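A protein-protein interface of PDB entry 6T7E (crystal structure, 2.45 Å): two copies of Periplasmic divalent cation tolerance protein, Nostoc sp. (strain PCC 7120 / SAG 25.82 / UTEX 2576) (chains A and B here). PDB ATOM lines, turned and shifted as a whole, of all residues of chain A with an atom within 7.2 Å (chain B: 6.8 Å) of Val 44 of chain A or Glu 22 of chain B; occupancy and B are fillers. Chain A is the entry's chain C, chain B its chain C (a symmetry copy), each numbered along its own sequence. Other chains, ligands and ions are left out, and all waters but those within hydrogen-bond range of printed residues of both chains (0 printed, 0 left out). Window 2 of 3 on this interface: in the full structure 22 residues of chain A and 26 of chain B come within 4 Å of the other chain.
The side-chain carboxylate of Glu 22 of chain B lies within salt-bridge range of the guanidinium group of Arg 18 of chain B.
The backbone carbonyl oxygen (O) of Tyr 38 of chain A is in hydrogen-bond range of the backbone NH (N) of Cys 45 of chain A (2.7 Å).
Among the printed residues, merely in contact across the chains: Ser 39 of chain A with His 24 of chain B, Ile 37 of chain A with Val 21 of chain B, Val 44 of chain A with Arg 18 of chain B, Ser 39 of chain A with Val 21 of chain B, Tyr 38 of chain A with Val 21 of chain B and Val 44 of chain A with Glu 22 of chain B.
Glu 22 of chain B touches one residue of chain A.
Printed residues of chain B within 4 Å of Ile 37 of chain A: Val 21.
Of the printed residues of chain A, Val 21 of chain B touches Ile 37 (3.5 Å), Tyr 38 (3.9 Å) and Ser 39 (3.8 Å).
Of the 10 printed residues of chain B, 4 touch a printed residue of chain A.
Printed residues of chain B that touch a printed residue of chain A: Arg 18, Val 21, Glu 22 and His 24.
Hydrophobic or aromatic side chains of chain B that line the printed part of chain A: Val 21 and His 24.
Along chain B the printed residues that touch a printed residue of chain A span positions 18 to 24.
Of the 10 printed residues of chain A, 4 touch a printed residue of chain B.
Hydrophobic or aromatic side chains of chain A that line the printed part of chain B: Ile 37 and Val 44.
Along chain A the printed residues that touch a printed residue of chain B span positions 37 to 44.
Among the printed residues, 6 pairs touch across the chains.
Among the printed residues, no Asp or Glu carboxylate lies within 4 Å of a Lys or Arg side-chain nitrogen of the other chain.
No position is printed for both chains.
Of the 6 pairs that touch across the chains among the printed residues, none has its exchanged pair printed and touching as well.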
ATOM      1  N   ILE A  37       8.439 -14.265  19.875  1.00  0.00           N
ATOM      2  CA  ILE A  37       9.641 -13.473  19.972  1.00  0.00           C
ATOM      3  C   ILE A  37       9.673 -12.609  18.715  1.00  0.00           C
ATOM      4  O   ILE A  37       9.705 -13.135  17.616  1.00  0.00           O
ATOM      5  CB  ILE A  37      10.893 -14.359  20.079  1.00  0.00           C
ATOM      6  CG1 ILE A  37      10.777 -15.306  21.271  1.00  0.00           C
ATOM      7  CG2 ILE A  37      12.143 -13.515  20.264  1.00  0.00           C
ATOM      8  CD1 ILE A  37      11.970 -16.223  21.456  1.00  0.00           C
ATOM      9  N   TYR A  38       9.624 -11.284  18.871  1.00  0.00           N
ATOM     10  CA  TYR A  38       9.659 -10.396  17.718  1.00  0.00           C
ATOM     11  C   TYR A  38      10.436  -9.121  17.981  1.00  0.00           C
ATOM     12  O   TYR A  38      10.619  -8.712  19.118  1.00  0.00           O
ATOM     13  CB  TYR A  38       8.245 -10.065  17.225  1.00  0.00           C
ATOM     14  CG  TYR A  38       7.345  -9.375  18.228  1.00  0.00           C
ATOM     15  CD1 TYR A  38       6.546 -10.099  19.096  1.00  0.00           C
ATOM     16  CD2 TYR A  38       7.264  -7.994  18.272  1.00  0.00           C
ATOM     17  CE1 TYR A  38       5.713  -9.463  20.002  1.00  0.00           C
ATOM     18  CE2 TYR A  38       6.433  -7.349  19.171  1.00  0.00           C
ATOM     19  CZ  TYR A  38       5.664  -8.083  20.040  1.00  0.00           C
ATOM     20  OH  TYR A  38       4.849  -7.413  20.932  1.00  0.00           O
ATOM     21  N   SER A  39      10.901  -8.527  16.890  1.00  0.00           N
ATOM     22  CA  SER A  39      11.650  -7.296  16.893  1.00  0.00           C
ATOM     23  C   SER A  39      10.654  -6.137  16.760  1.00  0.00           C
ATOM     24  O   SER A  39       9.782  -6.165  15.888  1.00  0.00           O
ATOM     25  CB  SER A  39      12.614  -7.319  15.702  1.00  0.00           C
ATOM     26  OG  SER A  39      13.511  -6.225  15.732  1.00  0.00           O
ATOM     27  N   TRP A  40      10.774  -5.126  17.618  1.00  0.00           N
ATOM     28  CA  TRP A  40       9.831  -3.998  17.614  1.00  0.00           C
ATOM     29  C   TRP A  40      10.450  -2.729  18.209  1.00  0.00           C
ATOM     30  O   TRP A  40      10.707  -2.652  19.412  1.00  0.00           O
ATOM     31  CB  TRP A  40       8.553  -4.388  18.370  1.00  0.00           C
ATOM     32  CG  TRP A  40       7.442  -3.378  18.321  1.00  0.00           C
ATOM     33  CD1 TRP A  40       6.977  -2.629  19.362  1.00  0.00           C
ATOM     34  CD2 TRP A  40       6.649  -3.016  17.183  1.00  0.00           C
ATOM     35  NE1 TRP A  40       5.954  -1.818  18.945  1.00  0.00           N
ATOM     36  CE2 TRP A  40       5.730  -2.031  17.611  1.00  0.00           C
ATOM     37  CE3 TRP A  40       6.631  -3.418  15.844  1.00  0.00           C
ATOM     38  CZ2 TRP A  40       4.797  -1.443  16.746  1.00  0.00           C
ATOM     39  CZ3 TRP A  40       5.702  -2.827  14.979  1.00  0.00           C
ATOM     40  CH2 TRP A  40       4.799  -1.849  15.439  1.00  0.00           C
ATOM     41  N   LYS A  41      10.687  -1.736  17.349  1.00  0.00           N
ATOM     42  CA  LYS A  41      11.248  -0.461  17.766  1.00  0.00           C
ATOM     43  C   LYS A  41      12.566  -0.666  18.514  1.00  0.00           C
ATOM     44  O   LYS A  41      12.796  -0.083  19.577  1.00  0.00           O
ATOM     45  CB  LYS A  41      10.237   0.318  18.615  1.00  0.00           C
ATOM     46  CG  LYS A  41       8.861   0.436  17.968  1.00  0.00           C
ATOM     47  CD  LYS A  41       7.964   1.414  18.718  1.00  0.00           C
ATOM     48  CE  LYS A  41       6.663   1.683  17.970  1.00  0.00           C
ATOM     49  NZ  LYS A  41       5.971   2.905  18.474  1.00  0.00           N
ATOM     50  N   GLY A  42      13.414  -1.518  17.947  1.00  0.00           N
ATOM     51  CA  GLY A  42      14.773  -1.722  18.437  1.00  0.00           C
ATOM     52  C   GLY A  42      14.878  -2.563  19.686  1.00  0.00           C
ATOM     53  O   GLY A  42      15.908  -2.544  20.365  1.00  0.00           O
ATOM     54  N   GLU A  43      13.818  -3.306  19.991  1.00  0.00           N
ATOM     55  CA  GLU A  43      13.795  -4.167  21.163  1.00  0.00           C
ATOM     56  C   GLU A  43      13.372  -5.561  20.761  1.00  0.00           C
ATOM     57  O   GLU A  43      12.478  -5.746  19.928  1.00  0.00           O
ATOM     58  CB  GLU A  43      12.819  -3.628  22.210  1.00  0.00           C
ATOM     59  CG  GLU A  43      13.193  -2.260  22.781  1.00  0.00           C
ATOM     60  CD  GLU A  43      14.258  -2.307  23.865  1.00  0.00           C
ATOM     61  OE1 GLU A  43      14.894  -1.262  24.103  1.00  0.00           O
ATOM     62  OE2 GLU A  43      14.461  -3.377  24.478  1.00  0.00           O
ATOM     63  N   VAL A  44      14.022  -6.546  21.355  1.00  0.00           N
ATOM     64  CA  VAL A  44      13.592  -7.922  21.230  1.00  0.00           C
ATOM     65  C   VAL A  44      12.477  -8.148  22.241  1.00  0.00           C
ATOM     66  O   VAL A  44      12.707  -8.051  23.449  1.00  0.00           O
ATOM     67  CB  VAL A  44      14.744  -8.892  21.505  1.00  0.00           C
ATOM     68  CG1 VAL A  44      14.247 -10.322  21.434  1.00  0.00           C
ATOM     69  CG2 VAL A  44      15.870  -8.647  20.505  1.00  0.00           C
ATOM     70  N   CYS A  45      11.281  -8.431  21.731  1.00  0.00           N
ATOM     71  CA  CYS A  45      10.078  -8.606  22.532  1.00  0.00           C
ATOM     72  C   CYS A  45       9.721 -10.080  22.681  1.00  0.00           C
ATOM     73  O   CYS A  45       9.846 -10.856  21.746  1.00  0.00           O
ATOM     74  CB  CYS A  45       8.910  -7.862  21.882  1.00  0.00           C
ATOM     75  SG  CYS A  45       9.175  -6.080  21.807  1.00  0.00           S
ATOM     76  N   SER A  46       9.257 -10.444  23.865  1.00  0.00           N
ATOM     77  CA  SER A  46       8.923 -11.808  24.208  1.00  0.00           C
ATOM     78  C   SER A  46       7.569 -11.741  24.870  1.00  0.00           C
ATOM     79  O   SER A  46       7.455 -11.162  25.948  1.00  0.00           O
ATOM     80  CB  SER A  46       9.957 -12.360  25.184  1.00  0.00           C
ATOM     81  OG  SER A  46       9.533 -13.585  25.755  1.00  0.00           O
ATOM     82  N   ALA B  17      15.509 -19.591  18.128  1.00  0.00           N
ATOM     83  CA  ALA B  17      14.523 -18.565  17.746  1.00  0.00           C
ATOM     84  C   ALA B  17      15.030 -17.175  18.107  1.00  0.00           C
ATOM     85  O   ALA B  17      15.088 -16.279  17.261  1.00  0.00           O
ATOM     86  CB  ALA B  17      13.190 -18.820  18.425  1.00  0.00           C
ATOM     87  N   ARG B  18      15.420 -17.032  19.369  1.00  0.00           N
ATOM     88  CA  ARG B  18      15.995 -15.802  19.912  1.00  0.00           C
ATOM     89  C   ARG B  18      17.118 -15.236  19.032  1.00  0.00           C
ATOM     90  O   ARG B  18      17.143 -14.042  18.729  1.00  0.00           O
ATOM     91  CB  ARG B  18      16.514 -16.087  21.329  1.00  0.00           C
ATOM     92  CG  ARG B  18      17.120 -14.902  22.051  1.00  0.00           C
ATOM     93  CD  ARG B  18      16.133 -14.199  22.960  1.00  0.00           C
ATOM     94  NE  ARG B  18      16.646 -12.883  23.338  1.00  0.00           N
ATOM     95  CZ  ARG B  18      16.037 -12.039  24.165  1.00  0.00           C
ATOM     96  NH1 ARG B  18      16.600 -10.863  24.433  1.00  0.00           N
ATOM     97  NH2 ARG B  18      14.874 -12.366  24.723  1.00  0.00           N
ATOM     98  N   LEU B  19      18.046 -16.100  18.634  1.00  0.00           N
ATOM     99  CA  LEU B  19      19.148 -15.695  17.780  1.00  0.00           C
ATOM    100  C   LEU B  19      18.643 -15.128  16.446  1.00  0.00           C
ATOM    101  O   LEU B  19      19.074 -14.055  16.022  1.00  0.00           O
ATOM    102  CB  LEU B  19      20.107 -16.866  17.523  1.00  0.00           C
ATOM    103  CG  LEU B  19      21.107 -17.285  18.608  1.00  0.00           C
ATOM    104  CD1 LEU B  19      21.991 -18.414  18.081  1.00  0.00           C
ATOM    105  CD2 LEU B  19      21.984 -16.126  19.075  1.00  0.00           C
ATOM    106  N   LEU B  20      17.726 -15.841  15.800  1.00  0.00           N
ATOM    107  CA  LEU B  20      17.243 -15.446  14.476  1.00  0.00           C
ATOM    108  C   LEU B  20      16.544 -14.097  14.490  1.00  0.00           C
ATOM    109  O   LEU B  20      16.605 -13.366  13.507  1.00  0.00           O
ATOM    110  CB  LEU B  20      16.284 -16.490  13.900  1.00  0.00           C
ATOM    111  CG  LEU B  20      16.860 -17.864  13.545  1.00  0.00           C
ATOM    112  CD1 LEU B  20      15.721 -18.786  13.161  1.00  0.00           C
ATOM    113  CD2 LEU B  20      17.877 -17.807  12.423  1.00  0.00           C
ATOM    114  N   VAL B  21      15.882 -13.776  15.598  1.00  0.00           N
ATOM    115  CA  VAL B  21      15.257 -12.470  15.774  1.00  0.00           C
ATOM    116  C   VAL B  21      16.300 -11.382  15.976  1.00  0.00           C
ATOM    117  O   VAL B  21      16.255 -10.356  15.290  1.00  0.00           O
ATOM    118  CB  VAL B  21      14.266 -12.463  16.950  1.00  0.00           C
ATOM    119  CG1 VAL B  21      13.739 -11.057  17.204  1.00  0.00           C
ATOM    120  CG2 VAL B  21      13.101 -13.411  16.667  1.00  0.00           C
ATOM    121  N   GLU B  22      17.230 -11.619  16.906  1.00  0.00           N
ATOM    122  CA  GLU B  22      18.346 -10.696  17.209  1.00  0.00           C
ATOM    123  C   GLU B  22      19.207 -10.347  16.006  1.00  0.00           C
ATOM    124  O   GLU B  22      19.615  -9.199  15.861  1.00  0.00           O
ATOM    125  CB  GLU B  22      19.279 -11.288  18.277  1.00  0.00           C
ATOM    126  CG  GLU B  22      18.820 -11.099  19.710  1.00  0.00           C
ATOM    127  CD  GLU B  22      19.617 -11.937  20.698  1.00  0.00           C
ATOM    128  OE1 GLU B  22      20.770 -12.308  20.375  1.00  0.00           O
ATOM    129  OE2 GLU B  22      19.085 -12.231  21.795  1.00  0.00           O
ATOM    130  N   GLU B  23      19.513 -11.348  15.177  1.00  0.00           N
ATOM    131  CA  GLU B  23      20.346 -11.160  13.968  1.00  0.00           C
ATOM    132  C   GLU B  23      19.536 -10.553  12.816  1.00  0.00           C
ATOM    133  O   GLU B  23      20.078 -10.315  11.746  1.00  0.00           O
ATOM    134  CB  GLU B  23      20.972 -12.495  13.508  1.00  0.00           C
ATOM    135  CG  GLU B  23      21.972 -13.096  14.492  1.00  0.00           C
ATOM    136  CD  GLU B  23      22.553 -14.447  14.058  1.00  0.00           C
ATOM    137  OE1 GLU B  23      22.231 -14.937  12.954  1.00  0.00           O
ATOM    138  OE2 GLU B  23      23.359 -15.022  14.828  1.00  0.00           O
ATOM    139  N   HIS B  24      18.243 -10.317  13.049  1.00  0.00           N
ATOM    140  CA  HIS B  24      17.323  -9.788  12.040  1.00  0.00           C
ATOM    141  C   HIS B  24      17.243 -10.669  10.807  1.00  0.00           C
ATOM    142  O   HIS B  24      17.238 -10.182   9.679  1.00  0.00           O
ATOM    143  CB  HIS B  24      17.676  -8.343  11.675  1.00  0.00           C
ATOM    144  CG  HIS B  24      17.266  -7.354  12.719  1.00  0.00           C
ATOM    145  ND1 HIS B  24      16.004  -6.798  12.761  1.00  0.00           N
ATOM    146  CD2 HIS B  24      17.944  -6.836  13.767  1.00  0.00           C
ATOM    147  CE1 HIS B  24      15.925  -5.973  13.789  1.00  0.00           C
ATOM    148  NE2 HIS B  24      17.090  -5.974  14.411  1.00  0.00           N
ATOM    149  N   ILE B  25      17.179 -11.973  11.045  1.00  0.00           N
ATOM    150  CA  ILE B  25      17.011 -12.960   9.991  1.00  0.00           C
ATOM    151  C   ILE B  25      15.531 -13.284   9.841  1.00  0.00           C
ATOM    152  O   ILE B  25      15.070 -13.700   8.786  1.00  0.00           O
ATOM    153  CB  ILE B  25      17.857 -14.211  10.291  1.00  0.00           C
ATOM    154  CG1 ILE B  25      19.336 -13.824  10.204  1.00  0.00           C
ATOM    155  CG2 ILE B  25      17.524 -15.337   9.322  1.00  0.00           C
ATOM    156  CD1 ILE B  25      20.312 -14.937  10.523  1.00  0.00           C
ATOM    157  N   VAL B  26      14.788 -13.085  10.916  1.00  0.00           N
ATOM    158  CA  VAL B  26      13.346 -13.168  10.873  1.00  0.00           C
ATOM    159  C   VAL B  26      12.827 -11.980  11.662  1.00  0.00           C
ATOM    160  O   VAL B  26      13.497 -11.515  12.582  1.00  0.00           O
ATOM    161  CB  VAL B  26      12.805 -14.492  11.486  1.00  0.00           C
ATOM    162  CG1 VAL B  26      13.372 -15.700  10.760  1.00  0.00           C
ATOM    163  CG2 VAL B  26      13.119 -14.584  12.969  1.00  0.00           C
